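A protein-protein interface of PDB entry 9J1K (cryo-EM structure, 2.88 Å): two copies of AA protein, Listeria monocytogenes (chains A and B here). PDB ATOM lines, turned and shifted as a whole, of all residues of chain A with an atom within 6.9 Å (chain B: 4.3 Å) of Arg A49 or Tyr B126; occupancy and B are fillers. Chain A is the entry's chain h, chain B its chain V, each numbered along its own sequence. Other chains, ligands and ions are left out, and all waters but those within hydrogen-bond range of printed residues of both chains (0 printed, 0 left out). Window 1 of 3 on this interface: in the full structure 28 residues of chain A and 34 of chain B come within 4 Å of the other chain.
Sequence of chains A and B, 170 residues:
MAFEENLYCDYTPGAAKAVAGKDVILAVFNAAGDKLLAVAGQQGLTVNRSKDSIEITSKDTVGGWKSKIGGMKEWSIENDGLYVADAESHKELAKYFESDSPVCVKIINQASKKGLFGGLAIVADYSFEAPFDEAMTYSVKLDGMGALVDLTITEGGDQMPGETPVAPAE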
ATOM      1  N   VAL A  47      17.400  20.880   8.650  1.00  0.00           N
ATOM      2  CA  VAL A  47      18.180  21.180   9.841  1.00  0.00           C
ATOM      3  C   VAL A  47      17.503  20.513  11.030  1.00  0.00           C
ATOM      4  O   VAL A  47      16.308  20.210  11.003  1.00  0.00           O
ATOM      5  CB  VAL A  47      18.332  22.698  10.089  1.00  0.00           C
ATOM      6  CG1 VAL A  47      18.736  23.417   8.811  1.00  0.00           C
ATOM      7  CG2 VAL A  47      17.051  23.278  10.649  1.00  0.00           C
ATOM      8  N   ASN A  48      18.287  20.270  12.080  1.00  0.00           N
ATOM      9  CA  ASN A  48      17.769  19.677  13.306  1.00  0.00           C
ATOM     10  C   ASN A  48      18.522  20.257  14.490  1.00  0.00           C
ATOM     11  O   ASN A  48      19.754  20.202  14.533  1.00  0.00           O
ATOM     12  CB  ASN A  48      17.913  18.148  13.305  1.00  0.00           C
ATOM     13  CG  ASN A  48      17.851  17.552  11.913  1.00  0.00           C
ATOM     14  OD1 ASN A  48      18.871  17.416  11.239  1.00  0.00           O
ATOM     15  ND2 ASN A  48      16.651  17.189  11.476  1.00  0.00           N
ATOM     16  N   ARG A  49      17.782  20.817  15.443  1.00  0.00           N
ATOM     17  CA  ARG A  49      18.334  21.270  16.711  1.00  0.00           C
ATOM     18  C   ARG A  49      17.496  20.671  17.827  1.00  0.00           C
ATOM     19  O   ARG A  49      16.267  20.794  17.813  1.00  0.00           O
ATOM     20  CB  ARG A  49      18.343  22.799  16.810  1.00  0.00           C
ATOM     21  CG  ARG A  49      18.823  23.503  15.552  1.00  0.00           C
ATOM     22  CD  ARG A  49      17.943  24.694  15.212  1.00  0.00           C
ATOM     23  NE  ARG A  49      17.969  25.708  16.260  1.00  0.00           N
ATOM     24  CZ  ARG A  49      16.949  26.499  16.562  1.00  0.00           C
ATOM     25  NH1 ARG A  49      15.801  26.427  15.909  1.00  0.00           N
ATOM     26  NH2 ARG A  49      17.085  27.386  17.544  1.00  0.00           N
ATOM     27  N   SER A  50      18.149  20.022  18.787  1.00  0.00           N
ATOM     28  CA  SER A  50      17.414  19.327  19.834  1.00  0.00           C
ATOM     29  C   SER A  50      18.175  19.429  21.145  1.00  0.00           C
ATOM     30  O   SER A  50      19.323  19.868  21.189  1.00  0.00           O
ATOM     31  CB  SER A  50      17.169  17.861  19.466  1.00  0.00           C
ATOM     32  OG  SER A  50      16.669  17.140  20.577  1.00  0.00           O
ATOM     33  N   LYS A  51      17.507  19.034  22.226  1.00  0.00           N
ATOM     34  CA  LYS A  51      18.155  18.941  23.524  1.00  0.00           C
ATOM     35  C   LYS A  51      17.454  17.874  24.347  1.00  0.00           C
ATOM     36  O   LYS A  51      16.299  17.522  24.094  1.00  0.00           O
ATOM     37  CB  LYS A  51      18.157  20.282  24.267  1.00  0.00           C
ATOM     38  CG  LYS A  51      16.789  20.884  24.511  1.00  0.00           C
ATOM     39  CD  LYS A  51      16.850  21.888  25.653  1.00  0.00           C
ATOM     40  CE  LYS A  51      15.546  22.649  25.794  1.00  0.00           C
ATOM     41  NZ  LYS A  51      14.391  21.835  25.334  1.00  0.00           N
ATOM     42  N   LYS A  73      22.104  20.606  24.570  1.00  0.00           N
ATOM     43  CA  LYS A  73      21.616  20.790  23.203  1.00  0.00           C
ATOM     44  C   LYS A  73      22.659  20.428  22.147  1.00  0.00           C
ATOM     45  O   LYS A  73      23.861  20.613  22.342  1.00  0.00           O
ATOM     46  CB  LYS A  73      21.159  22.228  22.954  1.00  0.00           C
ATOM     47  CG  LYS A  73      20.551  22.951  24.127  1.00  0.00           C
ATOM     48  CD  LYS A  73      19.904  24.236  23.644  1.00  0.00           C
ATOM     49  CE  LYS A  73      20.791  25.455  23.868  1.00  0.00           C
ATOM     50  NZ  LYS A  73      21.076  25.648  25.324  1.00  0.00           N
ATOM     51  N   GLU A  74      22.166  19.943  21.004  1.00  0.00           N
ATOM     52  CA  GLU A  74      22.984  19.537  19.869  1.00  0.00           C
ATOM     53  C   GLU A  74      22.280  19.928  18.575  1.00  0.00           C
ATOM     54  O   GLU A  74      21.075  20.198  18.556  1.00  0.00           O
ATOM     55  CB  GLU A  74      23.262  18.025  19.882  1.00  0.00           C
ATOM     56  CG  GLU A  74      22.042  17.173  19.582  1.00  0.00           C
ATOM     57  CD  GLU A  74      21.142  17.004  20.791  1.00  0.00           C
ATOM     58  OE1 GLU A  74      21.424  17.619  21.841  1.00  0.00           O
ATOM     59  OE2 GLU A  74      20.148  16.256  20.695  1.00  0.00           O
ATOM     60  N   TRP A  75      23.048  19.969  17.484  1.00  0.00           N
ATOM     61  CA  TRP A  75      22.494  20.373  16.199  1.00  0.00           C
ATOM     62  C   TRP A  75      23.231  19.686  15.056  1.00  0.00           C
ATOM     63  O   TRP A  75      24.424  19.377  15.155  1.00  0.00           O
ATOM     64  CB  TRP A  75      22.553  21.893  16.025  1.00  0.00           C
ATOM     65  CG  TRP A  75      23.926  22.425  15.768  1.00  0.00           C
ATOM     66  CD1 TRP A  75      24.836  22.834  16.697  1.00  0.00           C
ATOM     67  CD2 TRP A  75      24.539  22.622  14.492  1.00  0.00           C
ATOM     68  NE1 TRP A  75      25.982  23.271  16.077  1.00  0.00           N
ATOM     69  CE2 TRP A  75      25.823  23.150  14.720  1.00  0.00           C
ATOM     70  CE3 TRP A  75      24.126  22.399  13.175  1.00  0.00           C
ATOM     71  CZ2 TRP A  75      26.697  23.461  13.682  1.00  0.00           C
ATOM     72  CZ3 TRP A  75      24.996  22.706  12.147  1.00  0.00           C
ATOM     73  CH2 TRP A  75      26.266  23.230  12.405  1.00  0.00           C
ATOM     74  N   SER A  76      22.502  19.464  13.963  1.00  0.00           N
ATOM     75  CA  SER A  76      23.041  18.806  12.780  1.00  0.00           C
ATOM     76  C   SER A  76      22.213  19.190  11.562  1.00  0.00           C
ATOM     77  O   SER A  76      20.991  19.331  11.651  1.00  0.00           O
ATOM     78  CB  SER A  76      23.058  17.282  12.949  1.00  0.00           C
ATOM     79  OG  SER A  76      21.958  16.681  12.287  1.00  0.00           O
ATOM     80  N   PHE A 117      21.422  31.000  10.114  1.00  0.00           N
ATOM     81  CA  PHE A 117      22.147  30.217  11.106  1.00  0.00           C
ATOM     82  C   PHE A 117      23.637  30.227  10.803  1.00  0.00           C
ATOM     83  O   PHE A 117      24.049  30.334   9.647  1.00  0.00           O
ATOM     84  CB  PHE A 117      21.644  28.768  11.159  1.00  0.00           C
ATOM     85  CG  PHE A 117      20.178  28.648  11.450  1.00  0.00           C
ATOM     86  CD1 PHE A 117      19.674  29.002  12.689  1.00  0.00           C
ATOM     87  CD2 PHE A 117      19.304  28.179  10.484  1.00  0.00           C
ATOM     88  CE1 PHE A 117      18.325  28.891  12.960  1.00  0.00           C
ATOM     89  CE2 PHE A 117      17.953  28.067  10.750  1.00  0.00           C
ATOM     90  CZ  PHE A 117      17.464  28.424  11.990  1.00  0.00           C
ATOM     91  N   LEU A 148      25.233  26.795  17.792  1.00  0.00           N
ATOM     92  CA  LEU A 148      24.812  27.133  16.434  1.00  0.00           C
ATOM     93  C   LEU A 148      24.003  28.418  16.555  1.00  0.00           C
ATOM     94  O   LEU A 148      22.818  28.383  16.899  1.00  0.00           O
ATOM     95  CB  LEU A 148      23.998  26.008  15.802  1.00  0.00           C
ATOM     96  CG  LEU A 148      23.314  26.332  14.472  1.00  0.00           C
ATOM     97  CD1 LEU A 148      24.335  26.424  13.351  1.00  0.00           C
ATOM     98  CD2 LEU A 148      22.245  25.301  14.147  1.00  0.00           C
ATOM     99  N   ASP A 150      21.821  31.692  15.993  1.00  0.00           N
ATOM    100  CA  ASP A 150      20.657  32.006  15.169  1.00  0.00           C
ATOM    101  C   ASP A 150      20.816  33.437  14.675  1.00  0.00           C
ATOM    102  O   ASP A 150      20.622  34.392  15.432  1.00  0.00           O
ATOM    103  CB  ASP A 150      19.369  31.829  15.965  1.00  0.00           C
ATOM    104  CG  ASP A 150      19.057  30.375  16.253  1.00  0.00           C
ATOM    105  OD1 ASP A 150      19.910  29.692  16.855  1.00  0.00           O
ATOM    106  OD2 ASP A 150      17.954  29.919  15.885  1.00  0.00           O
ATOM    107  N   TYR B  83       7.054  28.303   8.064  1.00  0.00           N
ATOM    108  CA  TYR B  83       8.003  29.017   8.907  1.00  0.00           C
ATOM    109  C   TYR B  83       8.289  30.393   8.326  1.00  0.00           C
ATOM    110  O   TYR B  83       8.548  30.525   7.125  1.00  0.00           O
ATOM    111  CB  TYR B  83       9.311  28.235   9.049  1.00  0.00           C
ATOM    112  CG  TYR B  83      10.360  28.958   9.863  1.00  0.00           C
ATOM    113  CD1 TYR B  83      10.103  29.350  11.168  1.00  0.00           C
ATOM    114  CD2 TYR B  83      11.606  29.251   9.327  1.00  0.00           C
ATOM    115  CE1 TYR B  83      11.056  30.013  11.918  1.00  0.00           C
ATOM    116  CE2 TYR B  83      12.566  29.912  10.068  1.00  0.00           C
ATOM    117  CZ  TYR B  83      12.286  30.291  11.363  1.00  0.00           C
ATOM    118  OH  TYR B  83      13.238  30.949  12.106  1.00  0.00           O
ATOM    119  N   HIS B  90       8.041  33.120  16.271  1.00  0.00           N
ATOM    120  CA  HIS B  90       9.215  32.280  16.061  1.00  0.00           C
ATOM    121  C   HIS B  90      10.458  32.886  16.695  1.00  0.00           C
ATOM    122  O   HIS B  90      11.323  32.150  17.183  1.00  0.00           O
ATOM    123  CB  HIS B  90       9.425  32.036  14.568  1.00  0.00           C
ATOM    124  CG  HIS B  90       8.332  31.236  13.931  1.00  0.00           C
ATOM    125  ND1 HIS B  90       8.400  29.867  13.786  1.00  0.00           N
ATOM    126  CD2 HIS B  90       7.142  31.610  13.407  1.00  0.00           C
ATOM    127  CE1 HIS B  90       7.300  29.433  13.197  1.00  0.00           C
ATOM    128  NE2 HIS B  90       6.520  30.471  12.955  1.00  0.00           N
ATOM    129  N   LEU B  93      10.152  31.910  20.253  1.00  0.00           N
ATOM    130  CA  LEU B  93      10.474  30.494  20.396  1.00  0.00           C
ATOM    131  C   LEU B  93      11.979  30.265  20.354  1.00  0.00           C
ATOM    132  O   LEU B  93      12.516  29.474  21.137  1.00  0.00           O
ATOM    133  CB  LEU B  93       9.778  29.685  19.302  1.00  0.00           C
ATOM    134  CG  LEU B  93       8.291  29.404  19.510  1.00  0.00           C
ATOM    135  CD1 LEU B  93       7.777  28.434  18.458  1.00  0.00           C
ATOM    136  CD2 LEU B  93       8.041  28.863  20.909  1.00  0.00           C
ATOM    137  N   ALA B  94      12.676  30.946  19.441  1.00  0.00           N
ATOM    138  CA  ALA B  94      14.129  30.826  19.377  1.00  0.00           C
ATOM    139  C   ALA B  94      14.780  31.349  20.651  1.00  0.00           C
ATOM    140  O   ALA B  94      15.732  30.746  21.165  1.00  0.00           O
ATOM    141  CB  ALA B  94      14.664  31.571  18.155  1.00  0.00           C
ATOM    142  N   PHE B  97      14.259  28.740  23.325  1.00  0.00           N
ATOM    143  CA  PHE B  97      15.097  27.566  23.109  1.00  0.00           C
ATOM    144  C   PHE B  97      16.546  27.851  23.481  1.00  0.00           C
ATOM    145  O   PHE B  97      17.220  27.003  24.078  1.00  0.00           O
ATOM    146  CB  PHE B  97      14.988  27.108  21.655  1.00  0.00           C
ATOM    147  CG  PHE B  97      15.944  26.008  21.289  1.00  0.00           C
ATOM    148  CD1 PHE B  97      15.636  24.688  21.568  1.00  0.00           C
ATOM    149  CD2 PHE B  97      17.140  26.292  20.652  1.00  0.00           C
ATOM    150  CE1 PHE B  97      16.509  23.672  21.231  1.00  0.00           C
ATOM    151  CE2 PHE B  97      18.017  25.280  20.313  1.00  0.00           C
ATOM    152  CZ  PHE B  97      17.699  23.969  20.602  1.00  0.00           C
ATOM    153  N   ALA B 124      11.765  20.697  23.075  1.00  0.00           N
ATOM    154  CA  ALA B 124      12.812  19.699  22.889  1.00  0.00           C
ATOM    155  C   ALA B 124      13.421  19.776  21.496  1.00  0.00           C
ATOM    156  O   ALA B 124      14.624  19.546  21.331  1.00  0.00           O
ATOM    157  CB  ALA B 124      12.255  18.300  23.150  1.00  0.00           C
ATOM    158  N   ASP B 125      12.616  20.095  20.484  1.00  0.00           N
ATOM    159  CA  ASP B 125      13.071  20.094  19.102  1.00  0.00           C
ATOM    160  C   ASP B 125      12.631  21.366  18.392  1.00  0.00           C
ATOM    161  O   ASP B 125      11.556  21.909  18.659  1.00  0.00           O
ATOM    162  CB  ASP B 125      12.539  18.871  18.341  1.00  0.00           C
ATOM    163  CG  ASP B 125      13.143  18.740  16.959  1.00  0.00           C
ATOM    164  OD1 ASP B 125      14.387  18.755  16.849  1.00  0.00           O
ATOM    165  OD2 ASP B 125      12.374  18.623  15.982  1.00  0.00           O
ATOM    166  N   TYR B 126      13.481  21.827  17.475  1.00  0.00           N
ATOM    167  CA  TYR B 126      13.183  22.990  16.640  1.00  0.00           C
ATOM    168  C   TYR B 126      13.918  22.778  15.319  1.00  0.00           C
ATOM    169  O   TYR B 126      15.112  23.075  15.218  1.00  0.00           O
ATOM    170  CB  TYR B 126      13.609  24.283  17.323  1.00  0.00           C
ATOM    171  CG  TYR B 126      12.804  25.498  16.917  1.00  0.00           C
ATOM    172  CD1 TYR B 126      11.880  25.431  15.885  1.00  0.00           C
ATOM    173  CD2 TYR B 126      12.971  26.711  17.570  1.00  0.00           C
ATOM    174  CE1 TYR B 126      11.144  26.541  15.514  1.00  0.00           C
ATOM    175  CE2 TYR B 126      12.240  27.825  17.206  1.00  0.00           C
ATOM    176  CZ  TYR B 126      11.328  27.735  16.178  1.00  0.00           C
ATOM    177  OH  TYR B 126      10.598  28.841  15.811  1.00  0.00           O
ATOM    178  N   SER B 127      13.204  22.268  14.318  1.00  0.00           N
ATOM    179  CA  SER B 127      13.813  21.844  13.067  1.00  0.00           C
ATOM    180  C   SER B 127      13.088  22.467  11.884  1.00  0.00           C
ATOM    181  O   SER B 127      11.907  22.815  11.969  1.00  0.00           O
ATOM    182  CB  SER B 127      13.800  20.316  12.935  1.00  0.00           C
ATOM    183  OG  SER B 127      14.251  19.700  14.129  1.00  0.00           O
ATOM    184  N   PHE B 128      13.815  22.603  10.776  1.00  0.00           N
ATOM    185  CA  PHE B 128      13.277  23.164   9.547  1.00  0.00           C
ATOM    186  C   PHE B 128      13.746  22.333   8.361  1.00  0.00           C
ATOM    187  O   PHE B 128      14.805  21.701   8.405  1.00  0.00           O
ATOM    188  CB  PHE B 128      13.702  24.626   9.358  1.00  0.00           C
ATOM    189  CG  PHE B 128      13.620  25.449  10.612  1.00  0.00           C
ATOM    190  CD1 PHE B 128      12.398  25.890  11.085  1.00  0.00           C
ATOM    191  CD2 PHE B 128      14.763  25.780  11.318  1.00  0.00           C
ATOM    192  CE1 PHE B 128      12.318  26.646  12.238  1.00  0.00           C
ATOM    193  CE2 PHE B 128      14.688  26.534  12.471  1.00  0.00           C
ATOM    194  CZ  PHE B 128      13.464  26.969  12.931  1.00  0.00           C
ATOM    195  N   SER B 139       9.030  22.628  12.320  1.00  0.00           N
ATOM    196  CA  SER B 139       8.447  21.612  13.185  1.00  0.00           C
ATOM    197  C   SER B 139       9.013  21.783  14.586  1.00  0.00           C
ATOM    198  O   SER B 139      10.234  21.836  14.760  1.00  0.00           O
ATOM    199  CB  SER B 139       8.736  20.201  12.663  1.00  0.00           C
ATOM    200  OG  SER B 139      10.131  19.984  12.533  1.00  0.00           O
ATOM    201  N   VAL B 140       8.128  21.867  15.576  1.00  0.00           N
ATOM    202  CA  VAL B 140       8.503  22.048  16.971  1.00  0.00           C
ATOM    203  C   VAL B 140       7.845  20.952  17.796  1.00  0.00           C
ATOM    204  O   VAL B 140       6.690  20.585  17.555  1.00  0.00           O
ATOM    205  CB  VAL B 140       8.093  23.438  17.503  1.00  0.00           C
ATOM    206  CG1 VAL B 140       8.768  23.715  18.832  1.00  0.00           C
ATOM    207  CG2 VAL B 140       8.434  24.519  16.499  1.00  0.00           C
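No position is printed for both chains.
Printed residues of chain B within 4 Å of Val A47: Ser B127 and Phe B128. Arg A49 touches just these residues of chain B: Phe B97, Asp B125, Tyr B126, Ser B127 and Phe B128. Ser A76 touches none of the printed residues of chain B. Of the printed residues of chain A, Ala B124 touches Ser A50 (3.2 Å) and Lys A51 (3.1 Å). Printed residues of chain A within 4 Å of Asp B125: Arg A49 and Ser A50. Tyr B126 touches one residue of chain A. Of the printed residues of chain A, Ser B127 touches Val A47 (3.2 Å), Asn A48 (3.6 Å) and Arg A49 (3.9 Å). The nearest residue of chain B that does not touch Arg A49 is Ala B124 (4.1 Å).
O of Ser A50 lies within hydrogen-bond range of N of Glu A74 (2.8 Å). The side-chain amide oxygen (OD1) of Asn A48 sits close to the backbone carbonyl oxygen (O) of Ser A76 (2.9 Å). A ring nitrogen (ND1) of His B90 lies within hydrogen-bond range of the side-chain hydroxyl (OH) of Tyr B126, at 3.2 Å. The side-chain carboxylate (OD2) of Asp B125 sits at hydrogen-bond distance from the side-chain hydroxyl (OG) of Ser B127 (2.8 Å). The side-chain carboxylate (OD2) of Asp A150 lies within salt-bridge range of the guanidinium group (NH2) of Arg A49 (3.2 Å). The backbone carbonyl oxygen (O) of Ser B127 lies within hydrogen-bond range of the backbone NH (N) of Ser B139, 2.9 Å away.
The backbone carbonyl oxygen (O) of Phe B128 lies within hydrogen-bond range of the backbone NH (N) of Val A47 (2.7 Å). O of Ala B124 is in hydrogen-bond range of N of Lys A51, at 3.1 Å. The side-chain carboxylate of Asp B125 lies close to the backbone carbonyl oxygen of Arg A49 (2.9 Å). The backbone carbonyl oxygen (O) of Ala B124 lies close to the side-chain hydroxyl (OG) of Ser A50 (3.2 Å). N of Tyr B126 sits at hydrogen-bond distance from O of Arg A49 (3.0 Å).
Hydrophobic or aromatic side chains of chain A within 4 Å of the printed part of chain B: Val A47 and Phe A117. Of the 12 printed residues of chain B, 6 touch a printed residue of chain A. Hydrophobic or aromatic side chains of chain B that line the printed part of chain A: Phe B97, Tyr B126 and Phe B128. Among the printed residues, 13 pairs touch across the chains. Among the printed residues, no Asp or Glu carboxylate lies within 4 Å of a Lys or Arg side-chain nitrogen of the other chain.
Among the printed residues, pairs that only touch across the chains: Val A47 with Ser B127 (3.2 Å), Asn A48 with Ser B127 (3.6 Å), Arg A49 with Phe B97 (3.3 Å), Arg A49 with Ser B127 (3.9 Å), Arg A49 with Phe B128 (3.6 Å), Ser A50 with Asp B125 (3.9 Å), Lys A73 with Phe B97 (3.8 Å) and Phe A117 with Phe B128 (3.4 Å).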
